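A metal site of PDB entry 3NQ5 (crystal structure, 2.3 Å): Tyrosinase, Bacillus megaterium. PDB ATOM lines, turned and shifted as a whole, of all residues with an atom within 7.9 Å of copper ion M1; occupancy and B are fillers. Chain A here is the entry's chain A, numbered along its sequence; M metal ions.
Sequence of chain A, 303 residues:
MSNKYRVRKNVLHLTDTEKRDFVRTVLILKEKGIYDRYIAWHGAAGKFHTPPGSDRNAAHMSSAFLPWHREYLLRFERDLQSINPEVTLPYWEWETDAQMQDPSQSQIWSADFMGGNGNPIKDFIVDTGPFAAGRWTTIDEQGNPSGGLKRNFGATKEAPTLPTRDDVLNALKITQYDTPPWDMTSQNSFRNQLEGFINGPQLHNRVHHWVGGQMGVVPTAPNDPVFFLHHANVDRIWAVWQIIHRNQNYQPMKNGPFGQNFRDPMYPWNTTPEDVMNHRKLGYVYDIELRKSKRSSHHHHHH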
ATOM      1  N   HIS A  42      17.758  13.669 -17.867  1.00  0.00           N
ATOM      2  CA  HIS A  42      17.718  12.801 -16.674  1.00  0.00           C
ATOM      3  C   HIS A  42      18.760  11.691 -16.778  1.00  0.00           C
ATOM      4  O   HIS A  42      19.511  11.460 -15.836  1.00  0.00           O
ATOM      5  CB  HIS A  42      16.296  12.201 -16.550  1.00  0.00           C
ATOM      6  CG  HIS A  42      16.106  11.276 -15.391  1.00  0.00           C
ATOM      7  ND1 HIS A  42      15.922   9.921 -15.546  1.00  0.00           N
ATOM      8  CD2 HIS A  42      16.043  11.518 -14.055  1.00  0.00           C
ATOM      9  CE1 HIS A  42      15.770   9.353 -14.352  1.00  0.00           C
ATOM     10  NE2 HIS A  42      15.842  10.302 -13.437  1.00  0.00           N
ATOM     11  N   ALA A  59      21.637  13.892 -10.068  1.00  0.00           N
ATOM     12  CA  ALA A  59      20.194  13.859  -9.811  1.00  0.00           C
ATOM     13  C   ALA A  59      19.795  12.910  -8.699  1.00  0.00           C
ATOM     14  O   ALA A  59      18.743  13.094  -8.100  1.00  0.00           O
ATOM     15  CB  ALA A  59      19.431  13.526 -11.065  1.00  0.00           C
ATOM     16  N   HIS A  60      20.605  11.899  -8.417  1.00  0.00           N
ATOM     17  CA  HIS A  60      20.205  10.860  -7.472  1.00  0.00           C
ATOM     18  C   HIS A  60      21.277  10.530  -6.458  1.00  0.00           C
ATOM     19  O   HIS A  60      22.418  10.966  -6.576  1.00  0.00           O
ATOM     20  CB  HIS A  60      19.857   9.560  -8.218  1.00  0.00           C
ATOM     21  CG  HIS A  60      18.850   9.711  -9.324  1.00  0.00           C
ATOM     22  ND1 HIS A  60      19.109  10.420 -10.468  1.00  0.00           N
ATOM     23  CD2 HIS A  60      17.613   9.192  -9.475  1.00  0.00           C
ATOM     24  CE1 HIS A  60      18.056  10.347 -11.274  1.00  0.00           C
ATOM     25  NE2 HIS A  60      17.140   9.603 -10.691  1.00  0.00           N
ATOM     26  N   PHE A  65      19.269  15.340  -5.232  1.00  0.00           N
ATOM     27  CA  PHE A  65      18.136  14.595  -5.770  1.00  0.00           C
ATOM     28  C   PHE A  65      16.821  15.359  -5.696  1.00  0.00           C
ATOM     29  O   PHE A  65      16.037  15.376  -6.632  1.00  0.00           O
ATOM     30  CB  PHE A  65      17.991  13.259  -5.065  1.00  0.00           C
ATOM     31  CG  PHE A  65      16.629  12.648  -5.182  1.00  0.00           C
ATOM     32  CD1 PHE A  65      16.229  12.013  -6.352  1.00  0.00           C
ATOM     33  CD2 PHE A  65      15.743  12.685  -4.123  1.00  0.00           C
ATOM     34  CE1 PHE A  65      14.990  11.434  -6.437  1.00  0.00           C
ATOM     35  CE2 PHE A  65      14.509  12.106  -4.224  1.00  0.00           C
ATOM     36  CZ  PHE A  65      14.130  11.487  -5.382  1.00  0.00           C
ATOM     37  N   HIS A  69      15.095  17.457  -9.181  1.00  0.00           N
ATOM     38  CA  HIS A  69      13.802  17.122  -9.736  1.00  0.00           C
ATOM     39  C   HIS A  69      12.819  18.301  -9.658  1.00  0.00           C
ATOM     40  O   HIS A  69      11.968  18.452 -10.545  1.00  0.00           O
ATOM     41  CB  HIS A  69      13.246  15.866  -9.065  1.00  0.00           C
ATOM     42  CG  HIS A  69      13.927  14.593  -9.478  1.00  0.00           C
ATOM     43  ND1 HIS A  69      15.024  14.083  -8.814  1.00  0.00           N
ATOM     44  CD2 HIS A  69      13.670  13.733 -10.495  1.00  0.00           C
ATOM     45  CE1 HIS A  69      15.406  12.971  -9.403  1.00  0.00           C
ATOM     46  NE2 HIS A  69      14.610  12.731 -10.427  1.00  0.00           N
ATOM     47  N   GLU A 195      14.050   9.423  -0.575  1.00  0.00           N
ATOM     48  CA  GLU A 195      14.551   8.841  -1.803  1.00  0.00           C
ATOM     49  C   GLU A 195      14.311   7.348  -1.767  1.00  0.00           C
ATOM     50  O   GLU A 195      13.944   6.760  -2.777  1.00  0.00           O
ATOM     51  CB  GLU A 195      16.032   9.146  -1.976  1.00  0.00           C
ATOM     52  CG  GLU A 195      16.620   8.617  -3.257  1.00  0.00           C
ATOM     53  CD  GLU A 195      17.788   9.418  -3.768  1.00  0.00           C
ATOM     54  OE1 GLU A 195      18.342   9.070  -4.839  1.00  0.00           O
ATOM     55  OE2 GLU A 195      18.151  10.399  -3.089  1.00  0.00           O
ATOM     56  N   HIS A 204      10.259   6.776  -2.545  1.00  0.00           N
ATOM     57  CA  HIS A 204      10.570   7.091  -3.961  1.00  0.00           C
ATOM     58  C   HIS A 204      11.075   5.899  -4.794  1.00  0.00           C
ATOM     59  O   HIS A 204      10.541   5.636  -5.875  1.00  0.00           O
ATOM     60  CB  HIS A 204      11.592   8.232  -4.078  1.00  0.00           C
ATOM     61  CG  HIS A 204      12.234   8.330  -5.428  1.00  0.00           C
ATOM     62  ND1 HIS A 204      13.495   7.839  -5.700  1.00  0.00           N
ATOM     63  CD2 HIS A 204      11.780   8.853  -6.593  1.00  0.00           C
ATOM     64  CE1 HIS A 204      13.796   8.089  -6.955  1.00  0.00           C
ATOM     65  NE2 HIS A 204      12.779   8.689  -7.535  1.00  0.00           N
ATOM     66  N   ASN A 205      12.097   5.189  -4.319  1.00  0.00           N
ATOM     67  CA  ASN A 205      12.607   4.047  -5.066  1.00  0.00           C
ATOM     68  C   ASN A 205      11.546   2.966  -5.193  1.00  0.00           C
ATOM     69  O   ASN A 205      11.275   2.468  -6.289  1.00  0.00           O
ATOM     70  CB  ASN A 205      13.848   3.459  -4.404  1.00  0.00           C
ATOM     71  CG  ASN A 205      14.978   4.449  -4.284  1.00  0.00           C
ATOM     72  OD1 ASN A 205      15.725   4.446  -3.318  1.00  0.00           O
ATOM     73  ND2 ASN A 205      15.104   5.313  -5.274  1.00  0.00           N
ATOM     74  N   VAL A 207       8.507   3.020  -5.341  1.00  0.00           N
ATOM     75  CA  VAL A 207       7.489   3.332  -6.344  1.00  0.00           C
ATOM     76  C   VAL A 207       8.029   3.184  -7.751  1.00  0.00           C
ATOM     77  O   VAL A 207       7.311   2.745  -8.662  1.00  0.00           O
ATOM     78  CB  VAL A 207       6.905   4.748  -6.128  1.00  0.00           C
ATOM     79  CG1 VAL A 207       5.908   5.101  -7.223  1.00  0.00           C
ATOM     80  CG2 VAL A 207       6.247   4.797  -4.762  1.00  0.00           C
ATOM     81  N   HIS A 208       9.290   3.548  -7.933  1.00  0.00           N
ATOM     82  CA  HIS A 208       9.955   3.304  -9.196  1.00  0.00           C
ATOM     83  C   HIS A 208       9.987   1.798  -9.455  1.00  0.00           C
ATOM     84  O   HIS A 208       9.649   1.336 -10.556  1.00  0.00           O
ATOM     85  CB  HIS A 208      11.363   3.885  -9.192  1.00  0.00           C
ATOM     86  CG  HIS A 208      11.449   5.287  -9.698  1.00  0.00           C
ATOM     87  ND1 HIS A 208      11.182   5.629 -11.011  1.00  0.00           N
ATOM     88  CD2 HIS A 208      11.781   6.453  -9.075  1.00  0.00           C
ATOM     89  CE1 HIS A 208      11.345   6.928 -11.176  1.00  0.00           C
ATOM     90  NE2 HIS A 208      11.707   7.450 -10.022  1.00  0.00           N
ATOM     91  N   MET A 215      10.107   2.545 -15.933  1.00  0.00           N
ATOM     92  CA  MET A 215      10.052   3.332 -14.709  1.00  0.00           C
ATOM     93  C   MET A 215      10.934   2.783 -13.604  1.00  0.00           C
ATOM     94  O   MET A 215      11.289   3.500 -12.673  1.00  0.00           O
ATOM     95  CB  MET A 215       8.620   3.468 -14.223  1.00  0.00           C
ATOM     96  CG  MET A 215       7.895   4.685 -14.773  1.00  0.00           C
ATOM     97  SD  MET A 215       7.899   6.082 -13.646  1.00  0.00           S
ATOM     98  CE  MET A 215       9.619   6.354 -13.429  1.00  0.00           C
ATOM     99  N   VAL A 218      16.785   3.968 -13.729  1.00  0.00           N
ATOM    100  CA  VAL A 218      17.110   5.379 -13.749  1.00  0.00           C
ATOM    101  C   VAL A 218      17.195   5.941 -15.163  1.00  0.00           C
ATOM    102  O   VAL A 218      16.587   6.951 -15.466  1.00  0.00           O
ATOM    103  CB  VAL A 218      18.413   5.664 -12.966  1.00  0.00           C
ATOM    104  CG1 VAL A 218      18.835   7.114 -13.174  1.00  0.00           C
ATOM    105  CG2 VAL A 218      18.225   5.396 -11.506  1.00  0.00           C
ATOM    106  N   ALA A 221      13.461   5.765 -16.933  1.00  0.00           N
ATOM    107  CA  ALA A 221      12.282   6.134 -16.136  1.00  0.00           C
ATOM    108  C   ALA A 221      11.338   7.136 -16.829  1.00  0.00           C
ATOM    109  O   ALA A 221      10.153   6.857 -17.006  1.00  0.00           O
ATOM    110  CB  ALA A 221      12.680   6.592 -14.751  1.00  0.00           C
ATOM    111  N   PRO A 222      11.837   8.322 -17.195  1.00  0.00           N
ATOM    112  CA  PRO A 222      10.921   9.355 -17.722  1.00  0.00           C
ATOM    113  C   PRO A 222      10.310   9.036 -19.092  1.00  0.00           C
ATOM    114  O   PRO A 222       9.520   9.848 -19.575  1.00  0.00           O
ATOM    115  CB  PRO A 222      11.806  10.602 -17.823  1.00  0.00           C
ATOM    116  CG  PRO A 222      12.939  10.318 -16.906  1.00  0.00           C
ATOM    117  CD  PRO A 222      13.187   8.865 -16.984  1.00  0.00           C
ATOM    118  N   PHE A 227       6.227   9.198 -14.529  1.00  0.00           N
ATOM    119  CA  PHE A 227       7.424   9.674 -13.850  1.00  0.00           C
ATOM    120  C   PHE A 227       7.200  11.053 -13.249  1.00  0.00           C
ATOM    121  O   PHE A 227       7.633  11.340 -12.121  1.00  0.00           O
ATOM    122  CB  PHE A 227       8.610   9.707 -14.817  1.00  0.00           C
ATOM    123  CG  PHE A 227       9.894  10.148 -14.170  1.00  0.00           C
ATOM    124  CD1 PHE A 227      10.236  11.497 -14.135  1.00  0.00           C
ATOM    125  CD2 PHE A 227      10.735   9.225 -13.578  1.00  0.00           C
ATOM    126  CE1 PHE A 227      11.406  11.914 -13.548  1.00  0.00           C
ATOM    127  CE2 PHE A 227      11.900   9.621 -12.962  1.00  0.00           C
ATOM    128  CZ  PHE A 227      12.242  10.967 -12.957  1.00  0.00           C
ATOM    129  N   HIS A 230       4.628  11.050 -10.411  1.00  0.00           N
ATOM    130  CA  HIS A 230       5.248  10.466  -9.236  1.00  0.00           C
ATOM    131  C   HIS A 230       6.151  11.455  -8.521  1.00  0.00           C
ATOM    132  O   HIS A 230       6.193  11.508  -7.293  1.00  0.00           O
ATOM    133  CB  HIS A 230       6.090   9.273  -9.684  1.00  0.00           C
ATOM    134  CG  HIS A 230       6.965   8.710  -8.611  1.00  0.00           C
ATOM    135  ND1 HIS A 230       8.156   8.082  -8.884  1.00  0.00           N
ATOM    136  CD2 HIS A 230       6.819   8.676  -7.270  1.00  0.00           C
ATOM    137  CE1 HIS A 230       8.708   7.672  -7.752  1.00  0.00           C
ATOM    138  NE2 HIS A 230       7.915   8.026  -6.756  1.00  0.00           N
ATOM    139  N   HIS A 231       6.904  12.241  -9.277  1.00  0.00           N
ATOM    140  CA  HIS A 231       7.824  13.159  -8.634  1.00  0.00           C
ATOM    141  C   HIS A 231       7.139  14.401  -8.107  1.00  0.00           C
ATOM    142  O   HIS A 231       7.643  15.034  -7.170  1.00  0.00           O
ATOM    143  CB  HIS A 231       9.035  13.475  -9.514  1.00  0.00           C
ATOM    144  CG  HIS A 231      10.124  12.458  -9.381  1.00  0.00           C
ATOM    145  ND1 HIS A 231      11.038  12.499  -8.345  1.00  0.00           N
ATOM    146  CD2 HIS A 231      10.399  11.339 -10.087  1.00  0.00           C
ATOM    147  CE1 HIS A 231      11.851  11.462  -8.443  1.00  0.00           C
ATOM    148  NE2 HIS A 231      11.495  10.744  -9.495  1.00  0.00           N
ATOM    149  N   VAL A 234       6.534  13.352  -4.715  1.00  0.00           N
ATOM    150  CA  VAL A 234       7.797  13.463  -4.002  1.00  0.00           C
ATOM    151  C   VAL A 234       8.059  14.913  -3.612  1.00  0.00           C
ATOM    152  O   VAL A 234       8.397  15.216  -2.460  1.00  0.00           O
ATOM    153  CB  VAL A 234       8.945  13.032  -4.903  1.00  0.00           C
ATOM    154  CG1 VAL A 234      10.269  13.311  -4.217  1.00  0.00           C
ATOM    155  CG2 VAL A 234       8.821  11.561  -5.291  1.00  0.00           C
HETATM  156 CU    CU M   1      12.567   9.126  -9.535  1.00  0.00          CU
HETATM  157 CU    CU M   2      15.488   9.215 -11.642  1.00  0.00          CU
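The backbone NH of Phe 227 sits close to the side-chain sulfur of Met 215 (3.6 Å). ND1 of His 204 sits close to O of Glu 195. A ring nitrogen (ND1) of His 208 lies within hydrogen-bond range of the backbone carbonyl oxygen (O) of Met 215 (2.7 Å). ND1 of His 204 lies within hydrogen-bond range of ND2 of Asn 205.
Residues that only touch copper ion M1: Phe 227. Of the 18 residues printed, 4 come within 4 Å of copper ion M1.
A ring nitrogen (NE2) of His 231 is bound to copper ion M1. A ring nitrogen (NE2) of His 208 binds copper ion M1 (1.9 Å). NE2 of His 204 is bound to copper ion M1 (2.1 Å). Copper ion M1 has three donor atoms within binding distance.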
